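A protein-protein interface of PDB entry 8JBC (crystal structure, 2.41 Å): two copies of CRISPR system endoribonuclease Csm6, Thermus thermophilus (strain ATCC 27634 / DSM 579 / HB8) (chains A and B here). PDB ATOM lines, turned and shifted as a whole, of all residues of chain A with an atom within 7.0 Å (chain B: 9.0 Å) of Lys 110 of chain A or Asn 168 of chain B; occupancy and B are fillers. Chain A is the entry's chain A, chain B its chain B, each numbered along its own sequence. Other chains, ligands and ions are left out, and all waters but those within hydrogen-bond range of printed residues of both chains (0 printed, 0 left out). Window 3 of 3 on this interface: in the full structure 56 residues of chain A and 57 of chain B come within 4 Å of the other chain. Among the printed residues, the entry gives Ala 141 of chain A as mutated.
No position is printed for both chains.
Of the 5 pairs that touch across the chains among the printed residues, none has its exchanged pair printed and touching as well.
Among the printed residues, pairs that only touch across the chains: Ser 111 of chain A with Asp 167 of chain B, Val 113 of chain A with Leu 188 of chain B, Ala 141 of chain A with Thr 137 of chain B and Ala 142 of chain A with Tyr 165 of chain B.
The side-chain amino group of Lys 110 of chain A is in hydrogen-bond range of the backbone carbonyl oxygen of Asn 168 of chain B, 3.2 Å away.
Of chain B, only Asn 168 comes within 4 Å of Lys 110 of chain A.
Of chain A, only Lys 110 comes within 4 Å of Asn 168 of chain B.
Of the printed residues of chain A, Thr 137 of chain B touches Ala 141 (3.9 Å).
Printed residues of chain B within 4 Å of Ala 141 of chain A: Thr 137 (3.9 Å).
Of the printed residues of chain A, Tyr 165 of chain B touches Ala 142.
Thr 182 of chain B touches none of the printed residues of chain A.
Arg 179 of chain B touches none of the printed residues of chain A.
The nearest residue of chain A that does not touch Asn 168 of chain B is Ser 111 of chain A (5.9 Å).
Hydrophobic or aromatic side chains of chain A within 4 Å of the printed part of chain B: Val 113, Ala 141 and Ala 142.
Hydrophobic or aromatic side chains of chain B within 4 Å of the printed part of chain A: Tyr 165 and Leu 188.
N of Val 166 of chain B is in hydrogen-bond range of OG1 of Thr 137 of chain B (2.7 Å).
OG1 of Thr 140 of chain A sits close to N of Ala 142 of chain A, at 3.4 Å.
The backbone carbonyl oxygen of Lys 110 of chain A sits at hydrogen-bond distance from the side-chain hydroxyl of Thr 140 of chain A, at 3.0 Å.
NH1 of Arg 186 of chain B is in salt-bridge range of OD2 of Asp 167 of chain B (2.8 Å).
O of Lys 184 of chain B sits at hydrogen-bond distance from N of Asp 167 of chain B (3.0 Å).
The backbone NH (N) of Tyr 165 of chain B is in hydrogen-bond range of the backbone carbonyl oxygen (O) of Arg 186 of chain B (2.9 Å).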
ATOM      1  N   HIS A  84     -10.540 -16.561   4.923  1.00  0.00           N
ATOM      2  CA  HIS A  84     -11.766 -15.797   5.112  1.00  0.00           C
ATOM      3  C   HIS A  84     -12.499 -16.236   6.373  1.00  0.00           C
ATOM      4  O   HIS A  84     -12.519 -17.424   6.717  1.00  0.00           O
ATOM      5  CB  HIS A  84     -12.688 -15.967   3.904  1.00  0.00           C
ATOM      6  CG  HIS A  84     -13.129 -17.380   3.685  1.00  0.00           C
ATOM      7  ND1 HIS A  84     -14.294 -17.886   4.222  1.00  0.00           N
ATOM      8  CD2 HIS A  84     -12.554 -18.401   3.000  1.00  0.00           C
ATOM      9  CE1 HIS A  84     -14.421 -19.155   3.868  1.00  0.00           C
ATOM     10  NE2 HIS A  84     -13.377 -19.496   3.132  1.00  0.00           N
ATOM     11  N   THR A  85     -13.108 -15.263   7.049  1.00  0.00           N
ATOM     12  CA  THR A  85     -14.101 -15.549   8.070  1.00  0.00           C
ATOM     13  C   THR A  85     -15.294 -16.267   7.441  1.00  0.00           C
ATOM     14  O   THR A  85     -15.545 -16.131   6.241  1.00  0.00           O
ATOM     15  CB  THR A  85     -14.567 -14.251   8.728  1.00  0.00           C
ATOM     16  OG1 THR A  85     -15.356 -13.496   7.803  1.00  0.00           O
ATOM     17  CG2 THR A  85     -13.402 -13.416   9.135  1.00  0.00           C
ATOM     18  N   PRO A  86     -16.051 -17.036   8.223  1.00  0.00           N
ATOM     19  CA  PRO A  86     -17.255 -17.680   7.653  1.00  0.00           C
ATOM     20  C   PRO A  86     -18.249 -16.693   7.053  1.00  0.00           C
ATOM     21  O   PRO A  86     -18.963 -17.043   6.103  1.00  0.00           O
ATOM     22  CB  PRO A  86     -17.860 -18.430   8.851  1.00  0.00           C
ATOM     23  CG  PRO A  86     -16.741 -18.615   9.788  1.00  0.00           C
ATOM     24  CD  PRO A  86     -15.832 -17.421   9.627  1.00  0.00           C
ATOM     25  N   GLU A  87     -18.320 -15.473   7.586  1.00  0.00           N
ATOM     26  CA  GLU A  87     -19.201 -14.459   7.022  1.00  0.00           C
ATOM     27  C   GLU A  87     -18.785 -14.091   5.606  1.00  0.00           C
ATOM     28  O   GLU A  87     -19.635 -13.924   4.722  1.00  0.00           O
ATOM     29  CB  GLU A  87     -19.195 -13.199   7.889  1.00  0.00           C
ATOM     30  CG  GLU A  87     -19.593 -13.383   9.359  1.00  0.00           C
ATOM     31  CD  GLU A  87     -18.609 -14.226  10.212  1.00  0.00           C
ATOM     32  OE1 GLU A  87     -18.578 -13.988  11.439  1.00  0.00           O
ATOM     33  OE2 GLU A  87     -17.895 -15.129   9.703  1.00  0.00           O
ATOM     34  N   ILE A 108     -11.435 -19.363   8.393  1.00  0.00           N
ATOM     35  CA  ILE A 108     -10.756 -19.018   9.644  1.00  0.00           C
ATOM     36  C   ILE A 108     -11.736 -18.218  10.501  1.00  0.00           C
ATOM     37  O   ILE A 108     -12.332 -17.253  10.013  1.00  0.00           O
ATOM     38  CB  ILE A 108      -9.490 -18.158   9.403  1.00  0.00           C
ATOM     39  CG1 ILE A 108      -8.225 -18.933   8.998  1.00  0.00           C
ATOM     40  CG2 ILE A 108      -9.131 -17.414  10.659  1.00  0.00           C
ATOM     41  CD1 ILE A 108      -8.310 -19.942   7.920  1.00  0.00           C
ATOM     42  N   GLY A 109     -11.864 -18.562  11.785  1.00  0.00           N
ATOM     43  CA  GLY A 109     -12.673 -17.736  12.675  1.00  0.00           C
ATOM     44  C   GLY A 109     -12.115 -16.327  12.805  1.00  0.00           C
ATOM     45  O   GLY A 109     -10.908 -16.099  12.693  1.00  0.00           O
ATOM     46  N   LYS A 110     -12.997 -15.355  13.055  1.00  0.00           N
ATOM     47  CA  LYS A 110     -12.538 -13.963  12.979  1.00  0.00           C
ATOM     48  C   LYS A 110     -11.584 -13.568  14.106  1.00  0.00           C
ATOM     49  O   LYS A 110     -10.994 -12.479  14.040  1.00  0.00           O
ATOM     50  CB  LYS A 110     -13.718 -12.988  12.958  1.00  0.00           C
ATOM     51  CG  LYS A 110     -14.906 -13.396  13.812  1.00  0.00           C
ATOM     52  CD  LYS A 110     -15.861 -12.212  13.998  1.00  0.00           C
ATOM     53  CE  LYS A 110     -15.220 -11.075  14.807  1.00  0.00           C
ATOM     54  NZ  LYS A 110     -15.033 -11.394  16.271  1.00  0.00           N
ATOM     55  N   SER A 111     -11.431 -14.395  15.139  1.00  0.00           N
ATOM     56  CA  SER A 111     -10.447 -14.136  16.191  1.00  0.00           C
ATOM     57  C   SER A 111      -9.724 -15.422  16.577  1.00  0.00           C
ATOM     58  O   SER A 111      -9.404 -15.647  17.749  1.00  0.00           O
ATOM     59  CB  SER A 111     -11.094 -13.467  17.413  1.00  0.00           C
ATOM     60  OG  SER A 111     -12.345 -14.055  17.759  1.00  0.00           O
ATOM     61  N   ASP A 112      -9.465 -16.290  15.601  1.00  0.00           N
ATOM     62  CA  ASP A 112      -8.658 -17.487  15.806  1.00  0.00           C
ATOM     63  C   ASP A 112      -7.301 -17.206  15.170  1.00  0.00           C
ATOM     64  O   ASP A 112      -6.999 -17.626  14.048  1.00  0.00           O
ATOM     65  CB  ASP A 112      -9.330 -18.743  15.218  1.00  0.00           C
ATOM     66  CG  ASP A 112      -8.644 -20.042  15.658  1.00  0.00           C
ATOM     67  OD1 ASP A 112      -7.658 -19.983  16.432  1.00  0.00           O
ATOM     68  OD2 ASP A 112      -9.090 -21.130  15.235  1.00  0.00           O
ATOM     69  N   VAL A 113      -6.466 -16.500  15.924  1.00  0.00           N
ATOM     70  CA  VAL A 113      -5.147 -16.138  15.426  1.00  0.00           C
ATOM     71  C   VAL A 113      -4.282 -17.372  15.241  1.00  0.00           C
ATOM     72  O   VAL A 113      -3.502 -17.473  14.271  1.00  0.00           O
ATOM     73  CB  VAL A 113      -4.509 -15.144  16.394  1.00  0.00           C
ATOM     74  CG1 VAL A 113      -3.020 -15.068  16.147  1.00  0.00           C
ATOM     75  CG2 VAL A 113      -5.206 -13.802  16.241  1.00  0.00           C
ATOM     76  N   GLY A 139      -9.405  -7.631   7.280  1.00  0.00           N
ATOM     77  CA  GLY A 139      -9.841  -8.516   8.342  1.00  0.00           C
ATOM     78  C   GLY A 139     -10.005  -7.728   9.627  1.00  0.00           C
ATOM     79  O   GLY A 139      -9.833  -6.511   9.663  1.00  0.00           O
ATOM     80  N   THR A 140     -10.318  -8.449  10.701  1.00  0.00           N
ATOM     81  CA  THR A 140     -10.288  -7.801  12.009  1.00  0.00           C
ATOM     82  C   THR A 140      -8.858  -7.371  12.335  1.00  0.00           C
ATOM     83  O   THR A 140      -7.890  -7.801  11.699  1.00  0.00           O
ATOM     84  CB  THR A 140     -10.825  -8.736  13.088  1.00  0.00           C
ATOM     85  OG1 THR A 140      -9.885  -9.792  13.322  1.00  0.00           O
ATOM     86  CG2 THR A 140     -12.153  -9.363  12.637  1.00  0.00           C
ATOM     87  N   ALA A 141      -8.725  -6.469  13.305  1.00  0.00           N
ATOM     88  CA  ALA A 141      -7.387  -6.057  13.711  1.00  0.00           C
ATOM     89  C   ALA A 141      -6.557  -7.263  14.144  1.00  0.00           C
ATOM     90  O   ALA A 141      -5.338  -7.287  13.942  1.00  0.00           O
ATOM     91  CB  ALA A 141      -7.457  -5.028  14.841  1.00  0.00           C
ATOM     92  N   ALA A 142      -7.205  -8.274  14.720  1.00  0.00           N
ATOM     93  CA  ALA A 142      -6.471  -9.446  15.172  1.00  0.00           C
ATOM     94  C   ALA A 142      -6.064 -10.292  13.996  1.00  0.00           C
ATOM     95  O   ALA A 142      -4.984 -10.884  14.004  1.00  0.00           O
ATOM     96  CB  ALA A 142      -7.302 -10.288  16.149  1.00  0.00           C
ATOM     97  N   MET A 143      -6.925 -10.380  12.982  1.00  0.00           N
ATOM     98  CA  MET A 143      -6.556 -11.104  11.773  1.00  0.00           C
ATOM     99  C   MET A 143      -5.320 -10.480  11.134  1.00  0.00           C
ATOM    100  O   MET A 143      -4.345 -11.177  10.829  1.00  0.00           O
ATOM    101  CB  MET A 143      -7.723 -11.111  10.793  1.00  0.00           C
ATOM    102  CG  MET A 143      -8.676 -12.290  10.915  1.00  0.00           C
ATOM    103  SD  MET A 143     -10.196 -12.065   9.928  1.00  0.00           S
ATOM    104  CE  MET A 143      -9.678 -12.680   8.319  1.00  0.00           C
ATOM    105  N   TYR B  29     -27.519   3.183  22.282  1.00  0.00           N
ATOM    106  CA  TYR B  29     -26.365   2.493  22.849  1.00  0.00           C
ATOM    107  C   TYR B  29     -25.481   3.447  23.653  1.00  0.00           C
ATOM    108  O   TYR B  29     -25.072   3.125  24.773  1.00  0.00           O
ATOM    109  CB  TYR B  29     -25.568   1.806  21.740  1.00  0.00           C
ATOM    110  CG  TYR B  29     -24.416   0.953  22.232  1.00  0.00           C
ATOM    111  CD1 TYR B  29     -24.629  -0.355  22.657  1.00  0.00           C
ATOM    112  CD2 TYR B  29     -23.113   1.445  22.247  1.00  0.00           C
ATOM    113  CE1 TYR B  29     -23.575  -1.148  23.085  1.00  0.00           C
ATOM    114  CE2 TYR B  29     -22.054   0.664  22.689  1.00  0.00           C
ATOM    115  CZ  TYR B  29     -22.289  -0.633  23.106  1.00  0.00           C
ATOM    116  OH  TYR B  29     -21.244  -1.424  23.539  1.00  0.00           O
ATOM    117  N   LEU B  37     -21.468  -0.053  30.373  1.00  0.00           N
ATOM    118  CA  LEU B  37     -20.328  -0.934  30.107  1.00  0.00           C
ATOM    119  C   LEU B  37     -19.023  -0.308  30.577  1.00  0.00           C
ATOM    120  O   LEU B  37     -18.161  -0.992  31.139  1.00  0.00           O
ATOM    121  CB  LEU B  37     -20.251  -1.243  28.613  1.00  0.00           C
ATOM    122  CG  LEU B  37     -19.153  -2.155  28.081  1.00  0.00           C
ATOM    123  CD1 LEU B  37     -19.230  -3.498  28.788  1.00  0.00           C
ATOM    124  CD2 LEU B  37     -19.281  -2.311  26.558  1.00  0.00           C
ATOM    125  N   TRP B  41     -16.085  -1.928  33.353  1.00  0.00           N
ATOM    126  CA  TRP B  41     -14.658  -1.971  33.077  1.00  0.00           C
ATOM    127  C   TRP B  41     -13.854  -1.049  33.991  1.00  0.00           C
ATOM    128  O   TRP B  41     -12.647  -1.263  34.150  1.00  0.00           O
ATOM    129  CB  TRP B  41     -14.407  -1.616  31.597  1.00  0.00           C
ATOM    130  CG  TRP B  41     -14.664  -2.763  30.631  1.00  0.00           C
ATOM    131  CD1 TRP B  41     -15.869  -3.343  30.328  1.00  0.00           C
ATOM    132  CD2 TRP B  41     -13.679  -3.478  29.879  1.00  0.00           C
ATOM    133  NE1 TRP B  41     -15.694  -4.360  29.419  1.00  0.00           N
ATOM    134  CE2 TRP B  41     -14.357  -4.467  29.130  1.00  0.00           C
ATOM    135  CE3 TRP B  41     -12.290  -3.381  29.768  1.00  0.00           C
ATOM    136  CZ2 TRP B  41     -13.688  -5.346  28.282  1.00  0.00           C
ATOM    137  CZ3 TRP B  41     -11.628  -4.254  28.929  1.00  0.00           C
ATOM    138  CH2 TRP B  41     -12.324  -5.223  28.197  1.00  0.00           C
ATOM    139  N   GLU B  66     -13.940   4.373  21.646  1.00  0.00           N
ATOM    140  CA  GLU B  66     -14.685   3.475  22.521  1.00  0.00           C
ATOM    141  C   GLU B  66     -13.901   2.234  22.917  1.00  0.00           C
ATOM    142  O   GLU B  66     -13.594   2.044  24.098  1.00  0.00           O
ATOM    143  CB  GLU B  66     -15.996   3.037  21.876  1.00  0.00           C
ATOM    144  CG  GLU B  66     -17.166   3.889  22.265  1.00  0.00           C
ATOM    145  CD  GLU B  66     -18.018   4.232  21.076  1.00  0.00           C
ATOM    146  OE1 GLU B  66     -18.341   3.307  20.302  1.00  0.00           O
ATOM    147  OE2 GLU B  66     -18.340   5.426  20.902  1.00  0.00           O
ATOM    148  N   ALA B  67     -13.581   1.375  21.945  1.00  0.00           N
ATOM    149  CA  ALA B  67     -12.893   0.134  22.283  1.00  0.00           C
ATOM    150  C   ALA B  67     -11.524   0.411  22.900  1.00  0.00           C
ATOM    151  O   ALA B  67     -11.105  -0.298  23.820  1.00  0.00           O
ATOM    152  CB  ALA B  67     -12.778  -0.760  21.050  1.00  0.00           C
ATOM    153  N   THR B  68     -10.841   1.461  22.449  1.00  0.00           N
ATOM    154  CA  THR B  68      -9.572   1.809  23.060  1.00  0.00           C
ATOM    155  C   THR B  68      -9.756   2.107  24.540  1.00  0.00           C
ATOM    156  O   THR B  68      -8.985   1.620  25.376  1.00  0.00           O
ATOM    157  CB  THR B  68      -8.945   2.993  22.321  1.00  0.00           C
ATOM    158  OG1 THR B  68      -8.775   2.653  20.943  1.00  0.00           O
ATOM    159  CG2 THR B  68      -7.598   3.381  22.897  1.00  0.00           C
ATOM    160  N   LEU B  70     -11.981   1.051  26.676  1.00  0.00           N
ATOM    161  CA  LEU B  70     -12.086  -0.230  27.370  1.00  0.00           C
ATOM    162  C   LEU B  70     -10.718  -0.883  27.571  1.00  0.00           C
ATOM    163  O   LEU B  70     -10.451  -1.467  28.627  1.00  0.00           O
ATOM    164  CB  LEU B  70     -13.009  -1.156  26.586  1.00  0.00           C
ATOM    165  CG  LEU B  70     -14.420  -1.332  27.158  1.00  0.00           C
ATOM    166  CD1 LEU B  70     -15.042  -0.003  27.579  1.00  0.00           C
ATOM    167  CD2 LEU B  70     -15.309  -2.055  26.154  1.00  0.00           C
ATOM    168  N   THR B 137      -6.143  -2.430  19.076  1.00  0.00           N
ATOM    169  CA  THR B 137      -7.564  -2.637  18.816  1.00  0.00           C
ATOM    170  C   THR B 137      -8.087  -1.671  17.755  1.00  0.00           C
ATOM    171  O   THR B 137      -8.864  -2.064  16.880  1.00  0.00           O
ATOM    172  CB  THR B 137      -8.361  -2.493  20.113  1.00  0.00           C
ATOM    173  OG1 THR B 137      -7.981  -3.528  21.032  1.00  0.00           O
ATOM    174  CG2 THR B 137      -9.859  -2.589  19.832  1.00  0.00           C
ATOM    175  N   TYR B 165      -5.521  -7.025  22.624  1.00  0.00           N
ATOM    176  CA  TYR B 165      -6.568  -6.411  21.818  1.00  0.00           C
ATOM    177  C   TYR B 165      -7.909  -6.721  22.447  1.00  0.00           C
ATOM    178  O   TYR B 165      -8.092  -7.782  23.049  1.00  0.00           O
ATOM    179  CB  TYR B 165      -6.556  -6.931  20.391  1.00  0.00           C
ATOM    180  CG  TYR B 165      -6.938  -8.392  20.315  1.00  0.00           C
ATOM    181  CD1 TYR B 165      -6.024  -9.388  20.655  1.00  0.00           C
ATOM    182  CD2 TYR B 165      -8.206  -8.779  19.896  1.00  0.00           C
ATOM    183  CE1 TYR B 165      -6.360 -10.726  20.575  1.00  0.00           C
ATOM    184  CE2 TYR B 165      -8.557 -10.107  19.808  1.00  0.00           C
ATOM    185  CZ  TYR B 165      -7.627 -11.083  20.159  1.00  0.00           C
ATOM    186  OH  TYR B 165      -7.964 -12.408  20.062  1.00  0.00           O
ATOM    187  N   VAL B 166      -8.858  -5.813  22.252  1.00  0.00           N
ATOM    188  CA  VAL B 166     -10.213  -5.998  22.764  1.00  0.00           C
ATOM    189  C   VAL B 166     -10.996  -6.848  21.774  1.00  0.00           C
ATOM    190  O   VAL B 166     -11.176  -6.454  20.617  1.00  0.00           O
ATOM    191  CB  VAL B 166     -10.902  -4.650  23.017  1.00  0.00           C
ATOM    192  CG1 VAL B 166     -12.324  -4.869  23.464  1.00  0.00           C
ATOM    193  CG2 VAL B 166     -10.136  -3.877  24.085  1.00  0.00           C
ATOM    194  N   ASP B 167     -11.458  -8.011  22.235  1.00  0.00           N
ATOM    195  CA  ASP B 167     -12.197  -8.983  21.435  1.00  0.00           C
ATOM    196  C   ASP B 167     -13.700  -8.764  21.598  1.00  0.00           C
ATOM    197  O   ASP B 167     -14.196  -8.648  22.724  1.00  0.00           O
ATOM    198  CB  ASP B 167     -11.815 -10.403  21.866  1.00  0.00           C
ATOM    199  CG  ASP B 167     -12.472 -11.494  21.022  1.00  0.00           C
ATOM    200  OD1 ASP B 167     -13.425 -11.218  20.261  1.00  0.00           O
ATOM    201  OD2 ASP B 167     -12.018 -12.653  21.116  1.00  0.00           O
ATOM    202  N   ASN B 168     -14.420  -8.716  20.474  1.00  0.00           N
ATOM    203  CA  ASN B 168     -15.894  -8.693  20.471  1.00  0.00           C
ATOM    204  C   ASN B 168     -16.462 -10.040  19.999  1.00  0.00           C
ATOM    205  O   ASN B 168     -16.673 -10.257  18.798  1.00  0.00           O
ATOM    206  CB  ASN B 168     -16.441  -7.564  19.582  1.00  0.00           C
ATOM    207  CG  ASN B 168     -15.803  -6.226  19.878  1.00  0.00           C
ATOM    208  OD1 ASN B 168     -14.609  -6.038  19.661  1.00  0.00           O
ATOM    209  ND2 ASN B 168     -16.592  -5.291  20.390  1.00  0.00           N
ATOM    210  N   ARG B 177     -24.606  -5.474  16.283  1.00  0.00           N
ATOM    211  CA  ARG B 177     -23.676  -5.259  17.386  1.00  0.00           C
ATOM    212  C   ARG B 177     -23.516  -6.576  18.165  1.00  0.00           C
ATOM    213  O   ARG B 177     -24.401  -7.435  18.125  1.00  0.00           O
ATOM    214  CB  ARG B 177     -24.174  -4.122  18.302  1.00  0.00           C
ATOM    215  CG  ARG B 177     -23.483  -3.949  19.649  1.00  0.00           C
ATOM    216  CD  ARG B 177     -22.265  -2.997  19.600  1.00  0.00           C
ATOM    217  NE  ARG B 177     -22.458  -1.751  18.851  1.00  0.00           N
ATOM    218  CZ  ARG B 177     -23.465  -0.895  18.987  1.00  0.00           C
ATOM    219  NH1 ARG B 177     -24.479  -1.133  19.795  1.00  0.00           N
ATOM    220  NH2 ARG B 177     -23.455   0.234  18.283  1.00  0.00           N
ATOM    221  N   PRO B 178     -22.376  -6.766  18.829  1.00  0.00           N
ATOM    222  CA  PRO B 178     -22.266  -7.818  19.851  1.00  0.00           C
ATOM    223  C   PRO B 178     -22.926  -7.450  21.176  1.00  0.00           C
ATOM    224  O   PRO B 178     -23.034  -6.276  21.541  1.00  0.00           O
ATOM    225  CB  PRO B 178     -20.749  -7.963  20.034  1.00  0.00           C
ATOM    226  CG  PRO B 178     -20.193  -6.631  19.608  1.00  0.00           C
ATOM    227  CD  PRO B 178     -21.058  -6.225  18.454  1.00  0.00           C
ATOM    228  N   ARG B 179     -23.339  -8.494  21.911  1.00  0.00           N
ATOM    229  CA  ARG B 179     -23.947  -8.323  23.233  1.00  0.00           C
ATOM    230  C   ARG B 179     -22.972  -7.654  24.204  1.00  0.00           C
ATOM    231  O   ARG B 179     -21.823  -8.086  24.343  1.00  0.00           O
ATOM    232  CB  ARG B 179     -24.400  -9.678  23.778  1.00  0.00           C
ATOM    233  N   ALA B 180     -23.459  -6.627  24.919  1.00  0.00           N
ATOM    234  CA  ALA B 180     -22.608  -5.637  25.583  1.00  0.00           C
ATOM    235  C   ALA B 180     -21.877  -6.157  26.819  1.00  0.00           C
ATOM    236  O   ALA B 180     -21.112  -5.396  27.423  1.00  0.00           O
ATOM    237  CB  ALA B 180     -23.428  -4.405  25.972  1.00  0.00           C
ATOM    238  N   GLY B 181     -22.097  -7.400  27.235  1.00  0.00           N
ATOM    239  CA  GLY B 181     -21.324  -7.952  28.330  1.00  0.00           C
ATOM    240  C   GLY B 181     -20.197  -8.893  27.950  1.00  0.00           C
ATOM    241  O   GLY B 181     -19.436  -9.300  28.831  1.00  0.00           O
ATOM    242  N   THR B 182     -20.048  -9.228  26.664  1.00  0.00           N
ATOM    243  CA  THR B 182     -19.212 -10.336  26.215  1.00  0.00           C
ATOM    244  C   THR B 182     -17.870  -9.895  25.625  1.00  0.00           C
ATOM    245  O   THR B 182     -17.197 -10.693  24.968  1.00  0.00           O
ATOM    246  CB  THR B 182     -19.984 -11.179  25.201  1.00  0.00           C
ATOM    247  OG1 THR B 182     -20.335 -10.371  24.069  1.00  0.00           O
ATOM    248  CG2 THR B 182     -21.251 -11.736  25.831  1.00  0.00           C
ATOM    249  N   GLU B 183     -17.472  -8.651  25.839  1.00  0.00           N
ATOM    250  CA  GLU B 183     -16.152  -8.184  25.447  1.00  0.00           C
ATOM    251  C   GLU B 183     -15.123  -8.597  26.493  1.00  0.00           C
ATOM    252  O   GLU B 183     -15.362  -8.487  27.701  1.00  0.00           O
ATOM    253  CB  GLU B 183     -16.120  -6.657  25.294  1.00  0.00           C
ATOM    254  CG  GLU B 183     -17.229  -5.979  24.459  1.00  0.00           C
ATOM    255  CD  GLU B 183     -18.643  -6.388  24.838  1.00  0.00           C
ATOM    256  OE1 GLU B 183     -18.971  -6.326  26.045  1.00  0.00           O
ATOM    257  OE2 GLU B 183     -19.417  -6.783  23.935  1.00  0.00           O
ATOM    258  N   LYS B 184     -13.969  -9.065  26.025  1.00  0.00           N
ATOM    259  CA  LYS B 184     -12.851  -9.375  26.900  1.00  0.00           C
ATOM    260  C   LYS B 184     -11.579  -8.767  26.330  1.00  0.00           C
ATOM    261  O   LYS B 184     -11.389  -8.725  25.110  1.00  0.00           O
ATOM    262  CB  LYS B 184     -12.660 -10.889  27.069  1.00  0.00           C
ATOM    263  CG  LYS B 184     -13.886 -11.667  27.479  1.00  0.00           C
ATOM    264  CD  LYS B 184     -13.700 -13.116  27.076  1.00  0.00           C
ATOM    265  CE  LYS B 184     -14.085 -14.075  28.190  1.00  0.00           C
ATOM    266  NZ  LYS B 184     -15.473 -14.585  28.093  1.00  0.00           N
ATOM    267  N   LEU B 185     -10.709  -8.298  27.226  1.00  0.00           N
ATOM    268  CA  LEU B 185      -9.352  -7.928  26.844  1.00  0.00           C
ATOM    269  C   LEU B 185      -8.528  -9.195  26.714  1.00  0.00           C
ATOM    270  O   LEU B 185      -8.498 -10.020  27.629  1.00  0.00           O
ATOM    271  CB  LEU B 185      -8.730  -6.987  27.871  1.00  0.00           C
ATOM    272  CG  LEU B 185      -7.403  -6.403  27.407  1.00  0.00           C
ATOM    273  CD1 LEU B 185      -7.519  -5.941  25.962  1.00  0.00           C
ATOM    274  CD2 LEU B 185      -7.014  -5.251  28.290  1.00  0.00           C
ATOM    275  N   ARG B 186      -7.902  -9.383  25.562  1.00  0.00           N
ATOM    276  CA  ARG B 186      -7.202 -10.623  25.292  1.00  0.00           C
ATOM    277  C   ARG B 186      -5.749 -10.327  24.970  1.00  0.00           C
ATOM    278  O   ARG B 186      -5.404  -9.230  24.522  1.00  0.00           O
ATOM    279  CB  ARG B 186      -7.841 -11.407  24.152  1.00  0.00           C
ATOM    280  CG  ARG B 186      -9.301 -11.749  24.368  1.00  0.00           C
ATOM    281  CD  ARG B 186      -9.708 -13.008  23.614  1.00  0.00           C
ATOM    282  NE  ARG B 186     -10.862 -13.654  24.236  1.00  0.00           N
ATOM    283  CZ  ARG B 186     -11.634 -14.568  23.655  1.00  0.00           C
ATOM    284  NH1 ARG B 186     -11.389 -15.009  22.429  1.00  0.00           N
ATOM    285  NH2 ARG B 186     -12.675 -15.059  24.325  1.00  0.00           N
ATOM    286  N   LEU B 188      -2.675 -11.291  22.633  1.00  0.00           N
ATOM    287  CA  LEU B 188      -2.432 -11.941  21.351  1.00  0.00           C
ATOM    288  C   LEU B 188      -1.201 -12.842  21.462  1.00  0.00           C
ATOM    289  O   LEU B 188      -0.096 -12.348  21.695  1.00  0.00           O
ATOM    290  CB  LEU B 188      -2.249 -10.891  20.258  1.00  0.00           C
ATOM    291  CG  LEU B 188      -2.156 -11.383  18.813  1.00  0.00           C
ATOM    292  CD1 LEU B 188      -3.478 -11.929  18.397  1.00  0.00           C
ATOM    293  CD2 LEU B 188      -1.746 -10.239  17.870  1.00  0.00           C
